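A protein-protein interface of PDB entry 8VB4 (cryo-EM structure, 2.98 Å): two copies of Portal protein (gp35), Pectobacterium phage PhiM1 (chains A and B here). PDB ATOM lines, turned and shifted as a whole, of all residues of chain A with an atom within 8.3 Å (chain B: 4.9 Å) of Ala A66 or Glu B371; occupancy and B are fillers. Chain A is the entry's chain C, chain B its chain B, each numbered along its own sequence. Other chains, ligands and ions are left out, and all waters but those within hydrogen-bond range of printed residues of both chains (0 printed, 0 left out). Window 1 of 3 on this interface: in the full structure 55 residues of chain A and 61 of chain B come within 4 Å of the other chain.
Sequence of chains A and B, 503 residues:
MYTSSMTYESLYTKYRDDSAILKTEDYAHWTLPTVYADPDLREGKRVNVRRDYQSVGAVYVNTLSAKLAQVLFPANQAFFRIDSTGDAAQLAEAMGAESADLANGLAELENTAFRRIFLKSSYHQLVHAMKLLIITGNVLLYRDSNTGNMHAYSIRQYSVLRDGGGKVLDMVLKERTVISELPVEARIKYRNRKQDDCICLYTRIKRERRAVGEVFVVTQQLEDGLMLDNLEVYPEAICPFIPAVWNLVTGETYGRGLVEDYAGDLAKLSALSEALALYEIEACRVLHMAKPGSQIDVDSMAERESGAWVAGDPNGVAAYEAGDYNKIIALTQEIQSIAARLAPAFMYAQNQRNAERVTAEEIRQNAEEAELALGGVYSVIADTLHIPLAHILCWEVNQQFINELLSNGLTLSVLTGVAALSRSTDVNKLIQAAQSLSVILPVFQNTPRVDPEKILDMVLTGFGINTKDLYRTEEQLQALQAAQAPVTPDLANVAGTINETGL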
ATOM      1  N   VAL A  59       6.498   8.110  29.070  1.00  0.00           N
ATOM      2  CA  VAL A  59       5.110   7.819  28.726  1.00  0.00           C
ATOM      3  C   VAL A  59       5.047   6.853  27.550  1.00  0.00           C
ATOM      4  O   VAL A  59       4.279   5.882  27.558  1.00  0.00           O
ATOM      5  CB  VAL A  59       4.350   9.123  28.424  1.00  0.00           C
ATOM      6  CG1 VAL A  59       2.922   8.822  28.003  1.00  0.00           C
ATOM      7  CG2 VAL A  59       4.364  10.036  29.638  1.00  0.00           C
ATOM      8  N   TYR A  60       5.858   7.104  26.517  1.00  0.00           N
ATOM      9  CA  TYR A  60       5.826   6.239  25.342  1.00  0.00           C
ATOM     10  C   TYR A  60       6.215   4.810  25.704  1.00  0.00           C
ATOM     11  O   TYR A  60       5.557   3.847  25.286  1.00  0.00           O
ATOM     12  CB  TYR A  60       6.758   6.793  24.261  1.00  0.00           C
ATOM     13  CG  TYR A  60       6.228   8.011  23.526  1.00  0.00           C
ATOM     14  CD1 TYR A  60       4.976   8.540  23.812  1.00  0.00           C
ATOM     15  CD2 TYR A  60       6.986   8.627  22.541  1.00  0.00           C
ATOM     16  CE1 TYR A  60       4.498   9.645  23.140  1.00  0.00           C
ATOM     17  CE2 TYR A  60       6.513   9.734  21.864  1.00  0.00           C
ATOM     18  CZ  TYR A  60       5.269  10.238  22.169  1.00  0.00           C
ATOM     19  OH  TYR A  60       4.794  11.340  21.498  1.00  0.00           O
ATOM     20  N   VAL A  61       7.279   4.652  26.495  1.00  0.00           N
ATOM     21  CA  VAL A  61       7.745   3.317  26.857  1.00  0.00           C
ATOM     22  C   VAL A  61       6.714   2.609  27.723  1.00  0.00           C
ATOM     23  O   VAL A  61       6.440   1.418  27.532  1.00  0.00           O
ATOM     24  CB  VAL A  61       9.112   3.401  27.558  1.00  0.00           C
ATOM     25  CG1 VAL A  61       9.499   2.047  28.120  1.00  0.00           C
ATOM     26  CG2 VAL A  61      10.171   3.900  26.592  1.00  0.00           C
ATOM     27  N   ASN A  62       6.135   3.315  28.698  1.00  0.00           N
ATOM     28  CA  ASN A  62       5.106   2.705  29.532  1.00  0.00           C
ATOM     29  C   ASN A  62       3.943   2.213  28.683  1.00  0.00           C
ATOM     30  O   ASN A  62       3.487   1.071  28.830  1.00  0.00           O
ATOM     31  CB  ASN A  62       4.614   3.704  30.580  1.00  0.00           C
ATOM     32  CG  ASN A  62       5.553   3.824  31.760  1.00  0.00           C
ATOM     33  OD1 ASN A  62       6.102   2.833  32.236  1.00  0.00           O
ATOM     34  ND2 ASN A  62       5.739   5.046  32.247  1.00  0.00           N
ATOM     35  N   THR A  63       3.452   3.063  27.779  1.00  0.00           N
ATOM     36  CA  THR A  63       2.312   2.677  26.954  1.00  0.00           C
ATOM     37  C   THR A  63       2.643   1.461  26.100  1.00  0.00           C
ATOM     38  O   THR A  63       1.865   0.502  26.039  1.00  0.00           O
ATOM     39  CB  THR A  63       1.880   3.849  26.074  1.00  0.00           C
ATOM     40  OG1 THR A  63       1.709   5.021  26.881  1.00  0.00           O
ATOM     41  CG2 THR A  63       0.573   3.534  25.366  1.00  0.00           C
ATOM     42  N   LEU A  64       3.802   1.475  25.435  1.00  0.00           N
ATOM     43  CA  LEU A  64       4.143   0.366  24.551  1.00  0.00           C
ATOM     44  C   LEU A  64       4.324  -0.931  25.332  1.00  0.00           C
ATOM     45  O   LEU A  64       3.854  -1.992  24.903  1.00  0.00           O
ATOM     46  CB  LEU A  64       5.406   0.697  23.756  1.00  0.00           C
ATOM     47  CG  LEU A  64       5.912  -0.402  22.818  1.00  0.00           C
ATOM     48  CD1 LEU A  64       4.840  -0.787  21.815  1.00  0.00           C
ATOM     49  CD2 LEU A  64       7.173   0.048  22.101  1.00  0.00           C
ATOM     50  N   SER A  65       5.005  -0.870  26.480  1.00  0.00           N
ATOM     51  CA  SER A  65       5.219  -2.075  27.273  1.00  0.00           C
ATOM     52  C   SER A  65       3.901  -2.639  27.782  1.00  0.00           C
ATOM     53  O   SER A  65       3.692  -3.858  27.767  1.00  0.00           O
ATOM     54  CB  SER A  65       6.155  -1.774  28.442  1.00  0.00           C
ATOM     55  OG  SER A  65       5.532  -0.926  29.390  1.00  0.00           O
ATOM     56  N   ALA A  66       2.998  -1.772  28.248  1.00  0.00           N
ATOM     57  CA  ALA A  66       1.701  -2.252  28.711  1.00  0.00           C
ATOM     58  C   ALA A  66       0.900  -2.861  27.566  1.00  0.00           C
ATOM     59  O   ALA A  66       0.230  -3.883  27.744  1.00  0.00           O
ATOM     60  CB  ALA A  66       0.922  -1.111  29.360  1.00  0.00           C
ATOM     61  N   LYS A  67       0.959  -2.246  26.383  1.00  0.00           N
ATOM     62  CA  LYS A  67       0.151  -2.718  25.263  1.00  0.00           C
ATOM     63  C   LYS A  67       0.663  -4.052  24.730  1.00  0.00           C
ATOM     64  O   LYS A  67      -0.125  -4.920  24.342  1.00  0.00           O
ATOM     65  CB  LYS A  67       0.135  -1.663  24.158  1.00  0.00           C
ATOM     66  CG  LYS A  67      -0.785  -1.990  22.998  1.00  0.00           C
ATOM     67  CD  LYS A  67      -0.683  -0.941  21.905  1.00  0.00           C
ATOM     68  CE  LYS A  67      -1.415   0.334  22.288  1.00  0.00           C
ATOM     69  NZ  LYS A  67      -1.453   1.316  21.171  1.00  0.00           N
ATOM     70  N   LEU A  68       1.985  -4.234  24.697  1.00  0.00           N
ATOM     71  CA  LEU A  68       2.543  -5.460  24.135  1.00  0.00           C
ATOM     72  C   LEU A  68       2.108  -6.705  24.896  1.00  0.00           C
ATOM     73  O   LEU A  68       1.980  -7.773  24.288  1.00  0.00           O
ATOM     74  CB  LEU A  68       4.071  -5.391  24.113  1.00  0.00           C
ATOM     75  CG  LEU A  68       4.748  -4.731  22.910  1.00  0.00           C
ATOM     76  CD1 LEU A  68       6.252  -4.894  23.016  1.00  0.00           C
ATOM     77  CD2 LEU A  68       4.247  -5.311  21.598  1.00  0.00           C
ATOM     78  N   ALA A  69       1.885  -6.601  26.206  1.00  0.00           N
ATOM     79  CA  ALA A  69       1.560  -7.785  26.996  1.00  0.00           C
ATOM     80  C   ALA A  69       0.210  -8.366  26.590  1.00  0.00           C
ATOM     81  O   ALA A  69       0.040  -9.589  26.532  1.00  0.00           O
ATOM     82  CB  ALA A  69       1.573  -7.438  28.483  1.00  0.00           C
ATOM     83  N   GLN A  70      -0.767  -7.503  26.311  1.00  0.00           N
ATOM     84  CA  GLN A  70      -2.100  -7.988  25.964  1.00  0.00           C
ATOM     85  C   GLN A  70      -2.092  -8.734  24.636  1.00  0.00           C
ATOM     86  O   GLN A  70      -2.813  -9.725  24.468  1.00  0.00           O
ATOM     87  CB  GLN A  70      -3.084  -6.821  25.919  1.00  0.00           C
ATOM     88  CG  GLN A  70      -3.088  -5.966  27.174  1.00  0.00           C
ATOM     89  CD  GLN A  70      -4.064  -4.811  27.087  1.00  0.00           C
ATOM     90  OE1 GLN A  70      -5.126  -4.927  26.480  1.00  0.00           O
ATOM     91  NE2 GLN A  70      -3.704  -3.689  27.699  1.00  0.00           N
ATOM     92  N   VAL A  71      -1.294  -8.267  23.674  1.00  0.00           N
ATOM     93  CA  VAL A  71      -1.276  -8.895  22.356  1.00  0.00           C
ATOM     94  C   VAL A  71      -0.618 -10.268  22.412  1.00  0.00           C
ATOM     95  O   VAL A  71      -1.133 -11.236  21.840  1.00  0.00           O
ATOM     96  CB  VAL A  71      -0.564  -7.976  21.347  1.00  0.00           C
ATOM     97  CG1 VAL A  71      -0.493  -8.638  19.982  1.00  0.00           C
ATOM     98  CG2 VAL A  71      -1.272  -6.632  21.261  1.00  0.00           C
ATOM     99  N   LEU A  72       0.520 -10.379  23.095  1.00  0.00           N
ATOM    100  CA  LEU A  72       1.272 -11.628  23.156  1.00  0.00           C
ATOM    101  C   LEU A  72       0.613 -12.682  24.037  1.00  0.00           C
ATOM    102  O   LEU A  72       0.650 -13.870  23.703  1.00  0.00           O
ATOM    103  CB  LEU A  72       2.692 -11.356  23.661  1.00  0.00           C
ATOM    104  CG  LEU A  72       3.605 -10.521  22.760  1.00  0.00           C
ATOM    105  CD1 LEU A  72       4.905 -10.222  23.464  1.00  0.00           C
ATOM    106  CD2 LEU A  72       3.898 -11.263  21.469  1.00  0.00           C
ATOM    107  N   TYR A 123       2.512 -12.266  35.606  1.00  0.00           N
ATOM    108  CA  TYR A 123       2.190 -11.249  34.609  1.00  0.00           C
ATOM    109  C   TYR A 123       3.007  -9.980  34.827  1.00  0.00           C
ATOM    110  O   TYR A 123       3.472  -9.353  33.864  1.00  0.00           O
ATOM    111  CB  TYR A 123       0.692 -10.950  34.662  1.00  0.00           C
ATOM    112  CG  TYR A 123       0.137 -10.290  33.425  1.00  0.00           C
ATOM    113  CD1 TYR A 123      -0.216 -11.043  32.315  1.00  0.00           C
ATOM    114  CD2 TYR A 123      -0.052  -8.919  33.373  1.00  0.00           C
ATOM    115  CE1 TYR A 123      -0.732 -10.445  31.185  1.00  0.00           C
ATOM    116  CE2 TYR A 123      -0.567  -8.312  32.247  1.00  0.00           C
ATOM    117  CZ  TYR A 123      -0.905  -9.079  31.157  1.00  0.00           C
ATOM    118  OH  TYR A 123      -1.421  -8.478  30.032  1.00  0.00           O
ATOM    119  N   HIS A 124       3.182  -9.578  36.085  1.00  0.00           N
ATOM    120  CA  HIS A 124       3.990  -8.400  36.378  1.00  0.00           C
ATOM    121  C   HIS A 124       5.428  -8.597  35.918  1.00  0.00           C
ATOM    122  O   HIS A 124       6.044  -7.681  35.355  1.00  0.00           O
ATOM    123  CB  HIS A 124       3.934  -8.099  37.875  1.00  0.00           C
ATOM    124  CG  HIS A 124       4.727  -6.898  38.283  1.00  0.00           C
ATOM    125  ND1 HIS A 124       4.829  -5.771  37.497  1.00  0.00           N
ATOM    126  CD2 HIS A 124       5.453  -6.646  39.399  1.00  0.00           C
ATOM    127  CE1 HIS A 124       5.586  -4.878  38.109  1.00  0.00           C
ATOM    128  NE2 HIS A 124       5.977  -5.385  39.265  1.00  0.00           N
ATOM    129  N   VAL A 127       5.600  -8.153  32.195  1.00  0.00           N
ATOM    130  CA  VAL A 127       5.595  -6.744  31.799  1.00  0.00           C
ATOM    131  C   VAL A 127       6.965  -6.119  32.043  1.00  0.00           C
ATOM    132  O   VAL A 127       7.475  -5.348  31.214  1.00  0.00           O
ATOM    133  CB  VAL A 127       4.484  -5.984  32.546  1.00  0.00           C
ATOM    134  CG1 VAL A 127       4.508  -4.509  32.179  1.00  0.00           C
ATOM    135  CG2 VAL A 127       3.124  -6.588  32.232  1.00  0.00           C
ATOM    136  N   HIS A 128       7.582  -6.432  33.184  1.00  0.00           N
ATOM    137  CA  HIS A 128       8.919  -5.917  33.462  1.00  0.00           C
ATOM    138  C   HIS A 128       9.921  -6.409  32.423  1.00  0.00           C
ATOM    139  O   HIS A 128      10.801  -5.654  31.990  1.00  0.00           O
ATOM    140  CB  HIS A 128       9.355  -6.328  34.867  1.00  0.00           C
ATOM    141  CG  HIS A 128      10.578  -5.614  35.352  1.00  0.00           C
ATOM    142  ND1 HIS A 128      10.647  -4.242  35.452  1.00  0.00           N
ATOM    143  CD2 HIS A 128      11.779  -6.083  35.765  1.00  0.00           C
ATOM    144  CE1 HIS A 128      11.838  -3.895  35.906  1.00  0.00           C
ATOM    145  NE2 HIS A 128      12.544  -4.992  36.105  1.00  0.00           N
ATOM    146  N   MET A 130       9.236  -7.149  29.320  1.00  0.00           N
ATOM    147  CA  MET A 130       8.988  -6.392  28.095  1.00  0.00           C
ATOM    148  C   MET A 130       9.650  -5.021  28.164  1.00  0.00           C
ATOM    149  O   MET A 130      10.261  -4.562  27.189  1.00  0.00           O
ATOM    150  CB  MET A 130       7.486  -6.254  27.856  1.00  0.00           C
ATOM    151  CG  MET A 130       6.793  -7.574  27.588  1.00  0.00           C
ATOM    152  SD  MET A 130       7.361  -8.372  26.079  1.00  0.00           S
ATOM    153  CE  MET A 130       6.536  -9.951  26.224  1.00  0.00           C
ATOM    154  N   LYS A 131       9.541  -4.351  29.312  1.00  0.00           N
ATOM    155  CA  LYS A 131      10.230  -3.072  29.477  1.00  0.00           C
ATOM    156  C   LYS A 131      11.733  -3.234  29.279  1.00  0.00           C
ATOM    157  O   LYS A 131      12.372  -2.451  28.560  1.00  0.00           O
ATOM    158  CB  LYS A 131       9.941  -2.485  30.859  1.00  0.00           C
ATOM    159  CG  LYS A 131       8.557  -1.894  31.019  1.00  0.00           C
ATOM    160  CD  LYS A 131       8.240  -1.651  32.484  1.00  0.00           C
ATOM    161  CE  LYS A 131       7.080  -0.687  32.655  1.00  0.00           C
ATOM    162  NZ  LYS A 131       6.753  -0.462  34.088  1.00  0.00           N
ATOM    163  N   ILE A 134      12.617  -3.710  25.654  1.00  0.00           N
ATOM    164  CA  ILE A 134      12.469  -2.504  24.848  1.00  0.00           C
ATOM    165  C   ILE A 134      13.611  -1.528  25.102  1.00  0.00           C
ATOM    166  O   ILE A 134      14.136  -0.927  24.158  1.00  0.00           O
ATOM    167  CB  ILE A 134      11.104  -1.844  25.107  1.00  0.00           C
ATOM    168  CG1 ILE A 134       9.986  -2.706  24.518  1.00  0.00           C
ATOM    169  CG2 ILE A 134      11.073  -0.443  24.511  1.00  0.00           C
ATOM    170  CD1 ILE A 134       8.595  -2.254  24.895  1.00  0.00           C
ATOM    171  N   ALA B 367     -10.333  -1.981  33.828  1.00  0.00           N
ATOM    172  CA  ALA B 367      -9.065  -2.508  34.321  1.00  0.00           C
ATOM    173  C   ALA B 367      -8.007  -2.523  33.226  1.00  0.00           C
ATOM    174  O   ALA B 367      -6.836  -2.228  33.485  1.00  0.00           O
ATOM    175  CB  ALA B 367      -9.267  -3.911  34.890  1.00  0.00           C
ATOM    176  N   GLU B 368      -8.392  -2.873  31.997  1.00  0.00           N
ATOM    177  CA  GLU B 368      -7.428  -2.871  30.900  1.00  0.00           C
ATOM    178  C   GLU B 368      -6.901  -1.464  30.638  1.00  0.00           C
ATOM    179  O   GLU B 368      -5.698  -1.262  30.425  1.00  0.00           O
ATOM    180  CB  GLU B 368      -8.068  -3.452  29.640  1.00  0.00           C
ATOM    181  N   GLU B 369      -7.790  -0.471  30.655  1.00  0.00           N
ATOM    182  CA  GLU B 369      -7.350   0.900  30.421  1.00  0.00           C
ATOM    183  C   GLU B 369      -6.503   1.409  31.582  1.00  0.00           C
ATOM    184  O   GLU B 369      -5.575   2.201  31.380  1.00  0.00           O
ATOM    185  CB  GLU B 369      -8.557   1.806  30.183  1.00  0.00           C
ATOM    186  CG  GLU B 369      -8.199   3.160  29.596  1.00  0.00           C
ATOM    187  CD  GLU B 369      -9.394   3.863  28.989  1.00  0.00           C
ATOM    188  OE1 GLU B 369     -10.534   3.406  29.221  1.00  0.00           O
ATOM    189  OE2 GLU B 369      -9.195   4.868  28.276  1.00  0.00           O
ATOM    190  N   ALA B 370      -6.801   0.967  32.807  1.00  0.00           N
ATOM    191  CA  ALA B 370      -5.932   1.298  33.932  1.00  0.00           C
ATOM    192  C   ALA B 370      -4.552   0.682  33.751  1.00  0.00           C
ATOM    193  O   ALA B 370      -3.534   1.322  34.039  1.00  0.00           O
ATOM    194  CB  ALA B 370      -6.565   0.828  35.242  1.00  0.00           C
ATOM    195  N   GLU B 371      -4.500  -0.563  33.277  1.00  0.00           N
ATOM    196  CA  GLU B 371      -3.225  -1.166  32.909  1.00  0.00           C
ATOM    197  C   GLU B 371      -2.474  -0.296  31.915  1.00  0.00           C
ATOM    198  O   GLU B 371      -1.277  -0.035  32.082  1.00  0.00           O
ATOM    199  CB  GLU B 371      -3.457  -2.555  32.313  1.00  0.00           C
ATOM    200  CG  GLU B 371      -2.281  -3.505  32.456  1.00  0.00           C
ATOM    201  CD  GLU B 371      -2.211  -4.166  33.816  1.00  0.00           C
ATOM    202  OE1 GLU B 371      -3.186  -4.044  34.584  1.00  0.00           O
ATOM    203  OE2 GLU B 371      -1.188  -4.812  34.120  1.00  0.00           O
ATOM    204  N   LEU B 372      -3.162   0.159  30.869  1.00  0.00           N
ATOM    205  CA  LEU B 372      -2.494   0.955  29.844  1.00  0.00           C
ATOM    206  C   LEU B 372      -1.974   2.271  30.415  1.00  0.00           C
ATOM    207  O   LEU B 372      -0.847   2.685  30.120  1.00  0.00           O
ATOM    208  CB  LEU B 372      -3.442   1.207  28.669  1.00  0.00           C
ATOM    209  CG  LEU B 372      -3.921  -0.046  27.933  1.00  0.00           C
ATOM    210  CD1 LEU B 372      -5.019   0.291  26.938  1.00  0.00           C
ATOM    211  CD2 LEU B 372      -2.757  -0.738  27.242  1.00  0.00           C
ATOM    212  N   ALA B 373      -2.783   2.948  31.233  1.00  0.00           N
ATOM    213  CA  ALA B 373      -2.380   4.251  31.754  1.00  0.00           C
ATOM    214  C   ALA B 373      -1.235   4.124  32.754  1.00  0.00           C
ATOM    215  O   ALA B 373      -0.224   4.828  32.647  1.00  0.00           O
ATOM    216  CB  ALA B 373      -3.576   4.949  32.401  1.00  0.00           C
ATOM    217  N   LEU B 374      -1.377   3.229  33.736  1.00  0.00           N
ATOM    218  CA  LEU B 374      -0.395   3.156  34.816  1.00  0.00           C
ATOM    219  C   LEU B 374       0.975   2.734  34.300  1.00  0.00           C
ATOM    220  O   LEU B 374       2.000   3.287  34.715  1.00  0.00           O
ATOM    221  CB  LEU B 374      -0.873   2.189  35.899  1.00  0.00           C
ATOM    222  CG  LEU B 374      -2.148   2.586  36.646  1.00  0.00           C
ATOM    223  CD1 LEU B 374      -2.797   1.363  37.267  1.00  0.00           C
ATOM    224  CD2 LEU B 374      -1.848   3.630  37.709  1.00  0.00           C
ATOM    225  N   GLY B 375       1.015   1.756  33.400  1.00  0.00           N
ATOM    226  CA  GLY B 375       2.263   1.254  32.865  1.00  0.00           C
ATOM    227  C   GLY B 375       2.710  -0.087  33.399  1.00  0.00           C
ATOM    228  O   GLY B 375       3.828  -0.511  33.085  1.00  0.00           O
ATOM    229  N   GLY B 376       1.885  -0.764  34.194  1.00  0.00           N
ATOM    230  CA  GLY B 376       2.218  -2.094  34.672  1.00  0.00           C
ATOM    231  C   GLY B 376       2.257  -2.225  36.181  1.00  0.00           C
ATOM    232  O   GLY B 376       2.839  -3.178  36.705  1.00  0.00           O
ATOM    233  N   TYR B 378      -0.829  -1.878  38.075  1.00  0.00           N
ATOM    234  CA  TYR B 378      -2.061  -2.558  38.459  1.00  0.00           C
ATOM    235  C   TYR B 378      -1.793  -4.033  38.735  1.00  0.00           C
ATOM    236  O   TYR B 378      -2.301  -4.595  39.713  1.00  0.00           O
ATOM    237  CB  TYR B 378      -3.107  -2.402  37.353  1.00  0.00           C
ATOM    238  CG  TYR B 378      -4.373  -3.210  37.556  1.00  0.00           C
ATOM    239  CD1 TYR B 378      -5.439  -2.699  38.281  1.00  0.00           C
ATOM    240  CD2 TYR B 378      -4.494  -4.492  37.038  1.00  0.00           C
ATOM    241  CE1 TYR B 378      -6.601  -3.431  38.464  1.00  0.00           C
ATOM    242  CE2 TYR B 378      -5.647  -5.233  37.222  1.00  0.00           C
ATOM    243  CZ  TYR B 378      -6.695  -4.700  37.938  1.00  0.00           C
ATOM    244  OH  TYR B 378      -7.838  -5.441  38.123  1.00  0.00           O
ATOM    245  N   SER B 379      -0.989  -4.671  37.883  1.00  0.00           N
ATOM    246  CA  SER B 379      -0.632  -6.067  38.104  1.00  0.00           C
ATOM    247  C   SER B 379       0.166  -6.240  39.389  1.00  0.00           C
ATOM    248  O   SER B 379      -0.049  -7.206  40.128  1.00  0.00           O
ATOM    249  CB  SER B 379       0.157  -6.603  36.911  1.00  0.00           C
ATOM    250  OG  SER B 379      -0.666  -6.708  35.763  1.00  0.00           O
ATOM    251  N   VAL B 418      -5.328  -9.022  36.120  1.00  0.00           N
ATOM    252  CA  VAL B 418      -6.364  -8.939  35.092  1.00  0.00           C
ATOM    253  C   VAL B 418      -6.558 -10.314  34.464  1.00  0.00           C
ATOM    254  O   VAL B 418      -6.681 -10.445  33.242  1.00  0.00           O
ATOM    255  CB  VAL B 418      -6.032  -7.866  34.033  1.00  0.00           C
ATOM    256  CG1 VAL B 418      -4.767  -8.208  33.245  1.00  0.00           C
ATOM    257  CG2 VAL B 418      -7.217  -7.653  33.096  1.00  0.00           C
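NZ of Lys A131 lies within hydrogen-bond range of O of Gly B375, at 3.1 Å. The backbone carbonyl oxygen (O) of Gly B376 sits at hydrogen-bond distance from a ring nitrogen (ND1) of His A124 (3.4 Å).
OE2 of Glu B371 lies within hydrogen-bond range of OG of Ser B379 (2.6 Å).
Among the printed residues, merely in contact across the chains: Gln A70 with Leu B372, Tyr A123 with Ser B379 and Ala A66 with Glu B371.
Ala A66 touches one residue of chain B. Printed residues of chain B within 4 Å of Gln A70: Leu B372 (3.1 Å). Of the printed residues of chain B, His A124 touches Gly B376. Ala B370 touches none of the printed residues of chain A. Of the printed residues of chain A, Glu B371 touches Ala A66 (3.7 Å). Printed residues of chain A within 4 Å of Leu B372: Gln A70 (3.1 Å). Of the printed residues of chain A, Gly B375 touches Lys A131. The nearest residue of chain B that does not touch Ala A66 is Leu B372 (4.02 Å). The nearest printed residue of chain B that does not touch His A124 is Ser B379 (4.2 Å).
Of the 21 printed residues of chain A, 5 touch a printed residue of chain B. Hydrophobic or aromatic side chains of chain B within 4 Å of the printed part of chain A: Leu B372. Along chain B the printed residues that touch a printed residue of chain A span positions 371 to 379. Among the printed residues, no Asp or Glu carboxylate lies within 4 Å of a Lys or Arg side-chain nitrogen of the other chain.
No position is printed for both chains. Of the 5 pairs that touch across the chains among the printed residues, none has its exchanged pair printed and touching as well.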
